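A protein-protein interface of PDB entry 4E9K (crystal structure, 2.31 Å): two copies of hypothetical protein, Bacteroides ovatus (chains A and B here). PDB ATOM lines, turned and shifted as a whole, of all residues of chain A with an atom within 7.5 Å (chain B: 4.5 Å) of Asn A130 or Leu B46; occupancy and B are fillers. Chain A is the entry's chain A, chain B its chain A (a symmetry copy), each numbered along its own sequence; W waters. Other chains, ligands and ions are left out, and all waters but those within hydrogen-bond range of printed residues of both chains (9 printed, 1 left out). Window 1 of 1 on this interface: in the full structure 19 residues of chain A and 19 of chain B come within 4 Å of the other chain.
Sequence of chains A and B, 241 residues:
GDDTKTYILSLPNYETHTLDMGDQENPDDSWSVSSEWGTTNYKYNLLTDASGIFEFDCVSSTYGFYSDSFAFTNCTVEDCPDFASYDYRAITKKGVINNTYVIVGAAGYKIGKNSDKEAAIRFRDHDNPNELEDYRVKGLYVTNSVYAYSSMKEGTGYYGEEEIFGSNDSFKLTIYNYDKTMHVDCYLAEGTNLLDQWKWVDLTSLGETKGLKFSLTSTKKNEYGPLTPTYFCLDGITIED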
ATOM      1  N   ASP A  28      -3.334   6.411  36.516  1.00  0.00           N
ATOM      2  CA  ASP A  28      -2.840   7.698  36.064  1.00  0.00           C
ATOM      3  C   ASP A  28      -2.940   8.691  37.186  1.00  0.00           C
ATOM      4  O   ASP A  28      -2.082   9.521  37.331  1.00  0.00           O
ATOM      5  CB  ASP A  28      -3.646   8.205  34.867  1.00  0.00           C
ATOM      6  CG  ASP A  28      -3.412   7.378  33.624  1.00  0.00           C
ATOM      7  OD1 ASP A  28      -2.447   6.570  33.604  1.00  0.00           O
ATOM      8  OD2 ASP A  28      -4.190   7.532  32.666  1.00  0.00           O
ATOM      9  N   ASN A  45      -8.051   6.580  35.347  1.00  0.00           N
ATOM     10  CA  ASN A  45      -7.240   6.211  34.201  1.00  0.00           C
ATOM     11  C   ASN A  45      -7.882   6.741  32.932  1.00  0.00           C
ATOM     12  O   ASN A  45      -9.093   6.668  32.783  1.00  0.00           O
ATOM     13  CB  ASN A  45      -7.145   4.692  34.114  1.00  0.00           C
ATOM     14  CG  ASN A  45      -6.206   4.113  35.125  1.00  0.00           C
ATOM     15  OD1 ASN A  45      -5.027   4.444  35.104  1.00  0.00           O
ATOM     16  ND2 ASN A  45      -6.709   3.222  36.005  1.00  0.00           N
ATOM     17  N   LEU A  46      -7.077   7.272  32.018  1.00  0.00           N
ATOM     18  CA  LEU A  46      -7.553   7.624  30.699  1.00  0.00           C
ATOM     19  C   LEU A  46      -7.426   6.379  29.841  1.00  0.00           C
ATOM     20  O   LEU A  46      -6.342   6.001  29.448  1.00  0.00           O
ATOM     21  CB  LEU A  46      -6.708   8.750  30.123  1.00  0.00           C
ATOM     22  CG  LEU A  46      -7.104   9.355  28.774  1.00  0.00           C
ATOM     23  CD1 LEU A  46      -8.491  10.000  28.838  1.00  0.00           C
ATOM     24  CD2 LEU A  46      -6.061  10.384  28.356  1.00  0.00           C
ATOM     25  N   GLY A  52      -5.926   3.580  19.174  1.00  0.00           N
ATOM     26  CA  GLY A  52      -5.345   4.832  19.645  1.00  0.00           C
ATOM     27  C   GLY A  52      -6.079   6.087  19.227  1.00  0.00           C
ATOM     28  O   GLY A  52      -5.582   7.174  19.442  1.00  0.00           O
ATOM     29  N   GLU A  55     -10.223   7.937  23.372  1.00  0.00           N
ATOM     30  CA  GLU A  55      -9.872   7.921  24.732  1.00  0.00           C
ATOM     31  C   GLU A  55     -11.110   8.132  25.566  1.00  0.00           C
ATOM     32  O   GLU A  55     -12.039   8.807  25.130  1.00  0.00           O
ATOM     33  CB  GLU A  55      -8.788   8.994  25.001  1.00  0.00           C
ATOM     34  CG  GLU A  55      -9.272  10.425  25.136  1.00  0.00           C
ATOM     35  CD  GLU A  55      -8.172  11.409  25.440  1.00  0.00           C
ATOM     36  OE1 GLU A  55      -7.041  11.233  24.904  1.00  0.00           O
ATOM     37  OE2 GLU A  55      -8.436  12.375  26.211  1.00  0.00           O
ATOM     38  N   ARG A 124      -8.466  11.526  19.142  1.00  0.00           N
ATOM     39  CA  ARG A 124      -7.124  11.927  18.846  1.00  0.00           C
ATOM     40  C   ARG A 124      -6.828  11.800  17.360  1.00  0.00           C
ATOM     41  O   ARG A 124      -7.472  11.077  16.632  1.00  0.00           O
ATOM     42  CB  ARG A 124      -6.178  11.043  19.598  1.00  0.00           C
ATOM     43  CG  ARG A 124      -6.444  11.000  21.089  1.00  0.00           C
ATOM     44  CD  ARG A 124      -6.578   9.592  21.632  1.00  0.00           C
ATOM     45  NE  ARG A 124      -5.877   9.544  22.917  1.00  0.00           N
ATOM     46  CZ  ARG A 124      -4.876   8.739  23.193  1.00  0.00           C
ATOM     47  NH1 ARG A 124      -4.460   7.844  22.276  1.00  0.00           N
ATOM     48  NH2 ARG A 124      -4.298   8.822  24.396  1.00  0.00           N
ATOM     49  N   ASP A 125      -5.812  12.524  16.941  1.00  0.00           N
ATOM     50  CA  ASP A 125      -5.336  12.500  15.597  1.00  0.00           C
ATOM     51  C   ASP A 125      -4.762  11.121  15.321  1.00  0.00           C
ATOM     52  O   ASP A 125      -4.037  10.582  16.166  1.00  0.00           O
ATOM     53  CB  ASP A 125      -4.239  13.564  15.495  1.00  0.00           C
ATOM     54  CG  ASP A 125      -3.809  13.841  14.084  1.00  0.00           C
ATOM     55  OD1 ASP A 125      -3.337  12.916  13.416  1.00  0.00           O
ATOM     56  OD2 ASP A 125      -3.928  15.004  13.663  1.00  0.00           O
ATOM     57  N   ASP A 127      -2.467  10.385  13.243  1.00  0.00           N
ATOM     58  CA  ASP A 127      -1.010  10.470  13.102  1.00  0.00           C
ATOM     59  C   ASP A 127      -0.283  10.840  14.366  1.00  0.00           C
ATOM     60  O   ASP A 127       0.940  10.756  14.411  1.00  0.00           O
ATOM     61  CB  ASP A 127      -0.647  11.519  12.068  1.00  0.00           C
ATOM     62  CG  ASP A 127      -1.139  11.175  10.686  1.00  0.00           C
ATOM     63  OD1 ASP A 127      -1.241   9.968  10.351  1.00  0.00           O
ATOM     64  OD2 ASP A 127      -1.397  12.139   9.940  1.00  0.00           O
ATOM     65  N   ASN A 128      -1.015  11.287  15.381  1.00  0.00           N
ATOM     66  CA  ASN A 128      -0.390  11.700  16.635  1.00  0.00           C
ATOM     67  C   ASN A 128      -1.336  11.525  17.774  1.00  0.00           C
ATOM     68  O   ASN A 128      -2.236  12.332  17.955  1.00  0.00           O
ATOM     69  CB  ASN A 128       0.009  13.154  16.563  1.00  0.00           C
ATOM     70  CG  ASN A 128       0.726  13.600  17.788  1.00  0.00           C
ATOM     71  OD1 ASN A 128       1.082  12.803  18.642  1.00  0.00           O
ATOM     72  ND2 ASN A 128       0.945  14.881  17.884  1.00  0.00           N
ATOM     73  N   PRO A 129      -1.157  10.464  18.549  1.00  0.00           N
ATOM     74  CA  PRO A 129      -2.106  10.226  19.629  1.00  0.00           C
ATOM     75  C   PRO A 129      -2.064  11.286  20.726  1.00  0.00           C
ATOM     76  O   PRO A 129      -2.874  11.215  21.670  1.00  0.00           O
ATOM     77  CB  PRO A 129      -1.645   8.878  20.207  1.00  0.00           C
ATOM     78  CG  PRO A 129      -0.190   8.769  19.834  1.00  0.00           C
ATOM     79  CD  PRO A 129      -0.059   9.481  18.525  1.00  0.00           C
ATOM     80  N   ASN A 130      -1.109  12.219  20.633  1.00  0.00           N
ATOM     81  CA  ASN A 130      -0.917  13.234  21.668  1.00  0.00           C
ATOM     82  C   ASN A 130      -1.589  14.571  21.328  1.00  0.00           C
ATOM     83  O   ASN A 130      -1.349  15.577  21.958  1.00  0.00           O
ATOM     84  CB  ASN A 130       0.587  13.421  21.917  1.00  0.00           C
ATOM     85  CG  ASN A 130       1.272  12.126  22.284  1.00  0.00           C
ATOM     86  OD1 ASN A 130       2.116  11.620  21.536  1.00  0.00           O
ATOM     87  ND2 ASN A 130       0.851  11.542  23.388  1.00  0.00           N
ATOM     88  N   GLU A 131      -2.434  14.567  20.317  1.00  0.00           N
ATOM     89  CA  GLU A 131      -3.206  15.722  19.958  1.00  0.00           C
ATOM     90  C   GLU A 131      -4.657  15.290  19.753  1.00  0.00           C
ATOM     91  O   GLU A 131      -4.916  14.317  19.046  1.00  0.00           O
ATOM     92  CB  GLU A 131      -2.668  16.244  18.647  1.00  0.00           C
ATOM     93  CG  GLU A 131      -3.058  17.673  18.343  1.00  0.00           C
ATOM     94  CD  GLU A 131      -2.430  18.144  17.046  1.00  0.00           C
ATOM     95  OE1 GLU A 131      -2.178  17.312  16.120  1.00  0.00           O
ATOM     96  OE2 GLU A 131      -2.164  19.355  16.971  1.00  0.00           O
ATOM     97  N   LEU A 132      -5.593  16.013  20.358  1.00  0.00           N
ATOM     98  CA  LEU A 132      -7.008  15.865  20.052  1.00  0.00           C
ATOM     99  C   LEU A 132      -7.281  16.464  18.669  1.00  0.00           C
ATOM    100  O   LEU A 132      -6.580  17.359  18.224  1.00  0.00           O
ATOM    101  CB  LEU A 132      -7.889  16.539  21.125  1.00  0.00           C
ATOM    102  CG  LEU A 132      -7.692  16.071  22.582  1.00  0.00           C
ATOM    103  CD1 LEU A 132      -8.773  16.723  23.418  1.00  0.00           C
ATOM    104  CD2 LEU A 132      -7.755  14.547  22.770  1.00  0.00           C
ATOM    105  N   PRO B  12       5.843   9.465  16.723  1.00  0.00           N
ATOM    106  CA  PRO B  12       5.044   9.950  15.585  1.00  0.00           C
ATOM    107  C   PRO B  12       5.900  10.643  14.565  1.00  0.00           C
ATOM    108  O   PRO B  12       6.950  11.194  14.915  1.00  0.00           O
ATOM    109  CB  PRO B  12       4.085  10.962  16.227  1.00  0.00           C
ATOM    110  CG  PRO B  12       3.993  10.571  17.671  1.00  0.00           C
ATOM    111  CD  PRO B  12       5.311   9.926  18.020  1.00  0.00           C
ATOM    112  N   ASP B  20       6.493  18.477  20.677  1.00  0.00           N
ATOM    113  CA  ASP B  20       5.230  17.918  21.136  1.00  0.00           C
ATOM    114  C   ASP B  20       5.283  17.680  22.640  1.00  0.00           C
ATOM    115  O   ASP B  20       6.030  16.825  23.116  1.00  0.00           O
ATOM    116  CB  ASP B  20       4.911  16.641  20.368  1.00  0.00           C
ATOM    117  CG  ASP B  20       3.537  16.139  20.623  1.00  0.00           C
ATOM    118  OD1 ASP B  20       2.849  16.778  21.440  1.00  0.00           O
ATOM    119  OD2 ASP B  20       3.142  15.102  20.032  1.00  0.00           O
ATOM    120  N   GLY B  22       2.224  17.383  24.069  1.00  0.00           N
ATOM    121  CA  GLY B  22       0.832  17.025  24.155  1.00  0.00           C
ATOM    122  C   GLY B  22      -0.011  18.264  23.977  1.00  0.00           C
ATOM    123  O   GLY B  22       0.492  19.386  23.936  1.00  0.00           O
ATOM    124  N   ASP B  23      -1.308  18.027  23.884  1.00  0.00           N
ATOM    125  CA  ASP B  23      -2.302  19.054  23.686  1.00  0.00           C
ATOM    126  C   ASP B  23      -2.264  20.070  24.814  1.00  0.00           C
ATOM    127  O   ASP B  23      -2.421  19.747  25.992  1.00  0.00           O
ATOM    128  CB  ASP B  23      -3.684  18.405  23.589  1.00  0.00           C
ATOM    129  CG  ASP B  23      -4.678  19.255  22.823  1.00  0.00           C
ATOM    130  OD1 ASP B  23      -4.984  20.407  23.221  1.00  0.00           O
ATOM    131  OD2 ASP B  23      -5.158  18.752  21.810  1.00  0.00           O
ATOM    132  N   ASP B  28      -4.283  16.743  29.700  1.00  0.00           N
ATOM    133  CA  ASP B  28      -4.839  15.736  30.585  1.00  0.00           C
ATOM    134  C   ASP B  28      -5.084  16.344  31.936  1.00  0.00           C
ATOM    135  O   ASP B  28      -6.051  16.019  32.572  1.00  0.00           O
ATOM    136  CB  ASP B  28      -3.885  14.548  30.730  1.00  0.00           C
ATOM    137  CG  ASP B  28      -3.766  13.747  29.454  1.00  0.00           C
ATOM    138  OD1 ASP B  28      -4.601  13.945  28.532  1.00  0.00           O
ATOM    139  OD2 ASP B  28      -2.843  12.918  29.370  1.00  0.00           O
ATOM    140  N   TYR B  44      -0.056  19.111  32.202  1.00  0.00           N
ATOM    141  CA  TYR B  44       0.451  17.747  32.188  1.00  0.00           C
ATOM    142  C   TYR B  44      -0.270  16.938  31.116  1.00  0.00           C
ATOM    143  O   TYR B  44      -1.508  16.925  31.072  1.00  0.00           O
ATOM    144  CB  TYR B  44       0.195  17.030  33.542  1.00  0.00           C
ATOM    145  CG  TYR B  44       0.490  15.548  33.449  1.00  0.00           C
ATOM    146  CD1 TYR B  44       1.784  15.080  33.528  1.00  0.00           C
ATOM    147  CD2 TYR B  44      -0.526  14.617  33.212  1.00  0.00           C
ATOM    148  CE1 TYR B  44       2.076  13.730  33.416  1.00  0.00           C
ATOM    149  CE2 TYR B  44      -0.250  13.265  33.100  1.00  0.00           C
ATOM    150  CZ  TYR B  44       1.057  12.812  33.196  1.00  0.00           C
ATOM    151  OH  TYR B  44       1.360  11.449  33.064  1.00  0.00           O
ATOM    152  N   ASN B  45       0.511  16.214  30.312  1.00  0.00           N
ATOM    153  CA  ASN B  45      -0.008  15.235  29.375  1.00  0.00           C
ATOM    154  C   ASN B  45       0.797  13.953  29.480  1.00  0.00           C
ATOM    155  O   ASN B  45       2.012  14.002  29.592  1.00  0.00           O
ATOM    156  CB  ASN B  45       0.108  15.779  27.956  1.00  0.00           C
ATOM    157  CG  ASN B  45      -0.930  16.813  27.646  1.00  0.00           C
ATOM    158  OD1 ASN B  45      -2.115  16.508  27.707  1.00  0.00           O
ATOM    159  ND2 ASN B  45      -0.500  18.041  27.287  1.00  0.00           N
ATOM    160  N   LEU B  46       0.124  12.807  29.444  1.00  0.00           N
ATOM    161  CA  LEU B  46       0.799  11.533  29.339  1.00  0.00           C
ATOM    162  C   LEU B  46       0.999  11.266  27.858  1.00  0.00           C
ATOM    163  O   LEU B  46       0.069  10.933  27.153  1.00  0.00           O
ATOM    164  CB  LEU B  46      -0.051  10.438  29.962  1.00  0.00           C
ATOM    165  CG  LEU B  46       0.520   9.021  30.057  1.00  0.00           C
ATOM    166  CD1 LEU B  46       1.776   8.983  30.932  1.00  0.00           C
ATOM    167  CD2 LEU B  46      -0.543   8.084  30.616  1.00  0.00           C
ATOM    168  N   LEU B  47       2.213  11.411  27.376  1.00  0.00           N
ATOM    169  CA  LEU B  47       2.465  11.177  25.968  1.00  0.00           C
ATOM    170  C   LEU B  47       2.564   9.674  25.715  1.00  0.00           C
ATOM    171  O   LEU B  47       3.005   8.913  26.586  1.00  0.00           O
ATOM    172  CB  LEU B  47       3.751  11.876  25.527  1.00  0.00           C
ATOM    173  CG  LEU B  47       3.949  13.356  25.891  1.00  0.00           C
ATOM    174  CD1 LEU B  47       5.309  13.817  25.429  1.00  0.00           C
ATOM    175  CD2 LEU B  47       2.888  14.248  25.312  1.00  0.00           C
ATOM    176  N   THR B  48       2.137   9.237  24.538  1.00  0.00           N
ATOM    177  CA  THR B  48       2.344   7.869  24.116  1.00  0.00           C
ATOM    178  C   THR B  48       3.016   7.848  22.738  1.00  0.00           C
ATOM    179  O   THR B  48       2.882   8.774  21.945  1.00  0.00           O
ATOM    180  CB  THR B  48       1.023   7.072  24.112  1.00  0.00           C
ATOM    181  OG1 THR B  48       0.160   7.606  23.136  1.00  0.00           O
ATOM    182  CG2 THR B  48       0.291   7.143  25.457  1.00  0.00           C
ATOM    183  N   GLU B  55       4.783   5.147  27.276  1.00  0.00           N
ATOM    184  CA  GLU B  55       4.179   6.332  27.724  1.00  0.00           C
ATOM    185  C   GLU B  55       5.195   7.150  28.481  1.00  0.00           C
ATOM    186  O   GLU B  55       6.098   6.593  29.099  1.00  0.00           O
ATOM    187  CB  GLU B  55       2.938   5.989  28.584  1.00  0.00           C
ATOM    188  CG  GLU B  55       3.202   5.573  30.019  1.00  0.00           C
ATOM    189  CD  GLU B  55       1.948   5.298  30.809  1.00  0.00           C
ATOM    190  OE1 GLU B  55       0.975   4.746  30.221  1.00  0.00           O
ATOM    191  OE2 GLU B  55       1.933   5.621  32.031  1.00  0.00           O
ATOM    192  N   PHE B  56       4.991   8.474  28.469  1.00  0.00           N
ATOM    193  CA  PHE B  56       5.936   9.447  29.023  1.00  0.00           C
ATOM    194  C   PHE B  56       5.197  10.570  29.742  1.00  0.00           C
ATOM    195  O   PHE B  56       4.241  11.117  29.231  1.00  0.00           O
ATOM    196  CB  PHE B  56       6.714  10.136  27.906  1.00  0.00           C
ATOM    197  CG  PHE B  56       7.504   9.224  27.028  1.00  0.00           C
ATOM    198  CD1 PHE B  56       6.879   8.461  26.058  1.00  0.00           C
ATOM    199  CD2 PHE B  56       8.887   9.203  27.103  1.00  0.00           C
ATOM    200  CE1 PHE B  56       7.609   7.622  25.237  1.00  0.00           C
ATOM    201  CE2 PHE B  56       9.627   8.370  26.285  1.00  0.00           C
ATOM    202  CZ  PHE B  56       8.984   7.579  25.357  1.00  0.00           C
ATOM    203  N   ASP B  57       5.657  10.929  30.920  1.00  0.00           N
ATOM    204  CA  ASP B  57       5.115  12.058  31.654  1.00  0.00           C
ATOM    205  C   ASP B  57       5.632  13.379  31.089  1.00  0.00           C
ATOM    206  O   ASP B  57       6.843  13.604  31.064  1.00  0.00           O
ATOM    207  CB  ASP B  57       5.559  11.977  33.123  1.00  0.00           C
ATOM    208  CG  ASP B  57       4.912  10.838  33.886  1.00  0.00           C
ATOM    209  OD1 ASP B  57       3.683  10.575  33.706  1.00  0.00           O
ATOM    210  OD2 ASP B  57       5.628  10.253  34.731  1.00  0.00           O
ATOM    211  N   PHE B  72       8.564  15.057  22.815  1.00  0.00           N
ATOM    212  CA  PHE B  72       9.042  14.566  21.538  1.00  0.00           C
ATOM    213  C   PHE B  72       9.352  15.752  20.626  1.00  0.00           C
ATOM    214  O   PHE B  72       8.675  16.749  20.679  1.00  0.00           O
ATOM    215  CB  PHE B  72       8.007  13.701  20.812  1.00  0.00           C
ATOM    216  CG  PHE B  72       7.468  12.531  21.597  1.00  0.00           C
ATOM    217  CD1 PHE B  72       8.154  11.983  22.677  1.00  0.00           C
ATOM    218  CD2 PHE B  72       6.249  11.949  21.213  1.00  0.00           C
ATOM    219  CE1 PHE B  72       7.623  10.898  23.372  1.00  0.00           C
ATOM    220  CE2 PHE B  72       5.713  10.864  21.914  1.00  0.00           C
ATOM    221  CZ  PHE B  72       6.404  10.339  22.991  1.00  0.00           C
ATOM    222  N   ARG B 122       6.915   4.663  31.044  1.00  0.00           N
ATOM    223  CA  ARG B 122       6.338   3.397  31.463  1.00  0.00           C
ATOM    224  C   ARG B 122       5.917   2.574  30.286  1.00  0.00           C
ATOM    225  O   ARG B 122       5.665   3.104  29.194  1.00  0.00           O
ATOM    226  CB  ARG B 122       5.121   3.596  32.363  1.00  0.00           C
ATOM    227  CG  ARG B 122       5.343   4.308  33.670  1.00  0.00           C
ATOM    228  CD  ARG B 122       4.009   4.705  34.288  1.00  0.00           C
ATOM    229  NE  ARG B 122       4.284   5.833  35.121  1.00  0.00           N
ATOM    230  CZ  ARG B 122       4.173   7.099  34.770  1.00  0.00           C
ATOM    231  NH1 ARG B 122       3.654   7.454  33.606  1.00  0.00           N
ATOM    232  NH2 ARG B 122       4.538   8.011  35.644  1.00  0.00           N
HETATM  233  O   HOH W   1      -1.996   5.980  22.160  1.00  0.00           O
HETATM  234  O   HOH W   2      -2.425  15.358  24.792  1.00  0.00           O
HETATM  235  O   HOH W   3      -1.341   9.783  24.393  1.00  0.00           O
HETATM  236  O   HOH W   4      -0.920  13.129  25.483  1.00  0.00           O
HETATM  237  O   HOH W   5       0.240  17.434  20.814  1.00  0.00           O
HETATM  238  O   HOH W   6      -5.093  13.093  25.265  1.00  0.00           O
HETATM  239  O   HOH W   7      -1.224   4.049  31.657  1.00  0.00           O
HETATM  240  O   HOH W   8      -7.269  13.925  28.113  1.00  0.00           O
HETATM  241  O   HOH W   9       0.233   6.537  33.941  1.00  0.00           O
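Of the 15 printed residues of chain B, 9 touch a printed residue of chain A.
Hydrophobic or aromatic side chains of chain B that line the printed part of chain A: Pro B12, Leu B46, Leu B47 and Phe B72.
Among the printed residues, 14 pairs touch across the chains.
Among the printed residues, no Asp or Glu carboxylate lies within 4 Å of a Lys or Arg side-chain nitrogen of the other chain.
Water W5 lies within hydrogen-bond range of O of Asn A130, OD1 of Asp B20 and N of Asp B23.
Water W8 bridges the side-chain carboxylate of Asp B28 (2.7 Å) and the side-chain carboxylate of Glu A55 (2.7 Å).
Water W7 lies within hydrogen-bond range of OE1 of Glu B55 (2.7 Å) and OD1 of Asp A28 (3.4 Å).
Water W3 lies within hydrogen-bond range of OG1 of Thr B48 (2.9 Å), ND2 of Asn A130 (3.0 Å), NH2 of Arg A124 (3.1 Å), O of Leu B46 (3.3 Å) and O of Pro A129 (3.4 Å).
Water W4 bridges the backbone carbonyl oxygen (O) of Leu B46 (2.9 Å) and the side-chain amide nitrogen (ND2) of Asn A130 (3.2 Å).
Water W2 lies within hydrogen-bond range of N of Asp B23 (3.0 Å), O of Asn A130 (3.0 Å) and OD1 of Asn B45 (3.1 Å).
OD1 of Asp A28 touches CD2 of Leu B46, 3.9 Å away.
Leu A46 touches Asp B28 (CD2 to OD1, 3.9 Å).
O of Asp A127 touches CB of Pro B12, at 3.6 Å.
Pro B12 touches Asn A128 (CG to OD1, 3.8 Å).
Pro A129 touches Thr B48 (CG to OG1, 3.5 Å).
Asn A130 touches Asp B20 (CB to OD2, 3.6 Å).
Gly B22 touches Asn A130.
Asn A130 touches Leu B46 (ND2 to O, 3.9 Å).
Asn A130 touches Leu B47 (ND2 to CA, 3.1 Å).
Asn A130 touches Phe B72.
Of chain B, only Asp B20, Gly B22, Asp B23, Leu B46, Leu B47, Thr B48 and Phe B72 come within 4 Å of Asn A130.
Of the printed residues of chain A, Asp B23 touches Asn A130 and Leu A132.
Leu B46 touches just these residues of chain A: Asp A28 and Asn A130.
Of the printed residues of chain A, Leu B47 touches Asn A130.
The nearest residue of chain B that does not touch Asn A130 is Pro B12 (4.4 Å).
The nearest printed residue of chain A that does not touch Asp B28 is Glu A55 (4.7 Å).
The side-chain amide nitrogen (ND2) of Asn A128 lies within hydrogen-bond range of the side-chain carboxylate (OD2) of Asp B20.
The backbone NH (N) of Asp B23 sits at hydrogen-bond distance from the backbone carbonyl oxygen (O) of Asn A130 (3.1 Å).
N of Thr B48 sits close to ND2 of Asn A130 (2.9 Å).
N of Leu A132 is in hydrogen-bond range of OD2 of Asp B23 (3.1 Å).
Asp A28 touches Leu B46, and with the chains exchanged Leu A46 touches Asp B28.
OD1 of Asn A45 sits at hydrogen-bond distance from N of Asp A28, 3.0 Å away.
The side-chain carboxylate (OD2) of Asp A28 is in hydrogen-bond range of the backbone NH (N) of Leu A46, 3.0 Å away.
The side-chain carboxylate (OD1) of Asp A125 is in hydrogen-bond range of the backbone NH (N) of Asn A128 (3.5 Å).
The side-chain amide oxygen (OD1) of Asn A128 lies close to the backbone NH (N) of Asn A130, 3.0 Å away.
The backbone NH (N) of Asp B28 lies within hydrogen-bond range of the backbone carbonyl oxygen (O) of Tyr B44 (3.1 Å).
The side-chain carboxylate (OD2) of Asp B28 sits at hydrogen-bond distance from the backbone NH (N) of Leu B46 (3.0 Å).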
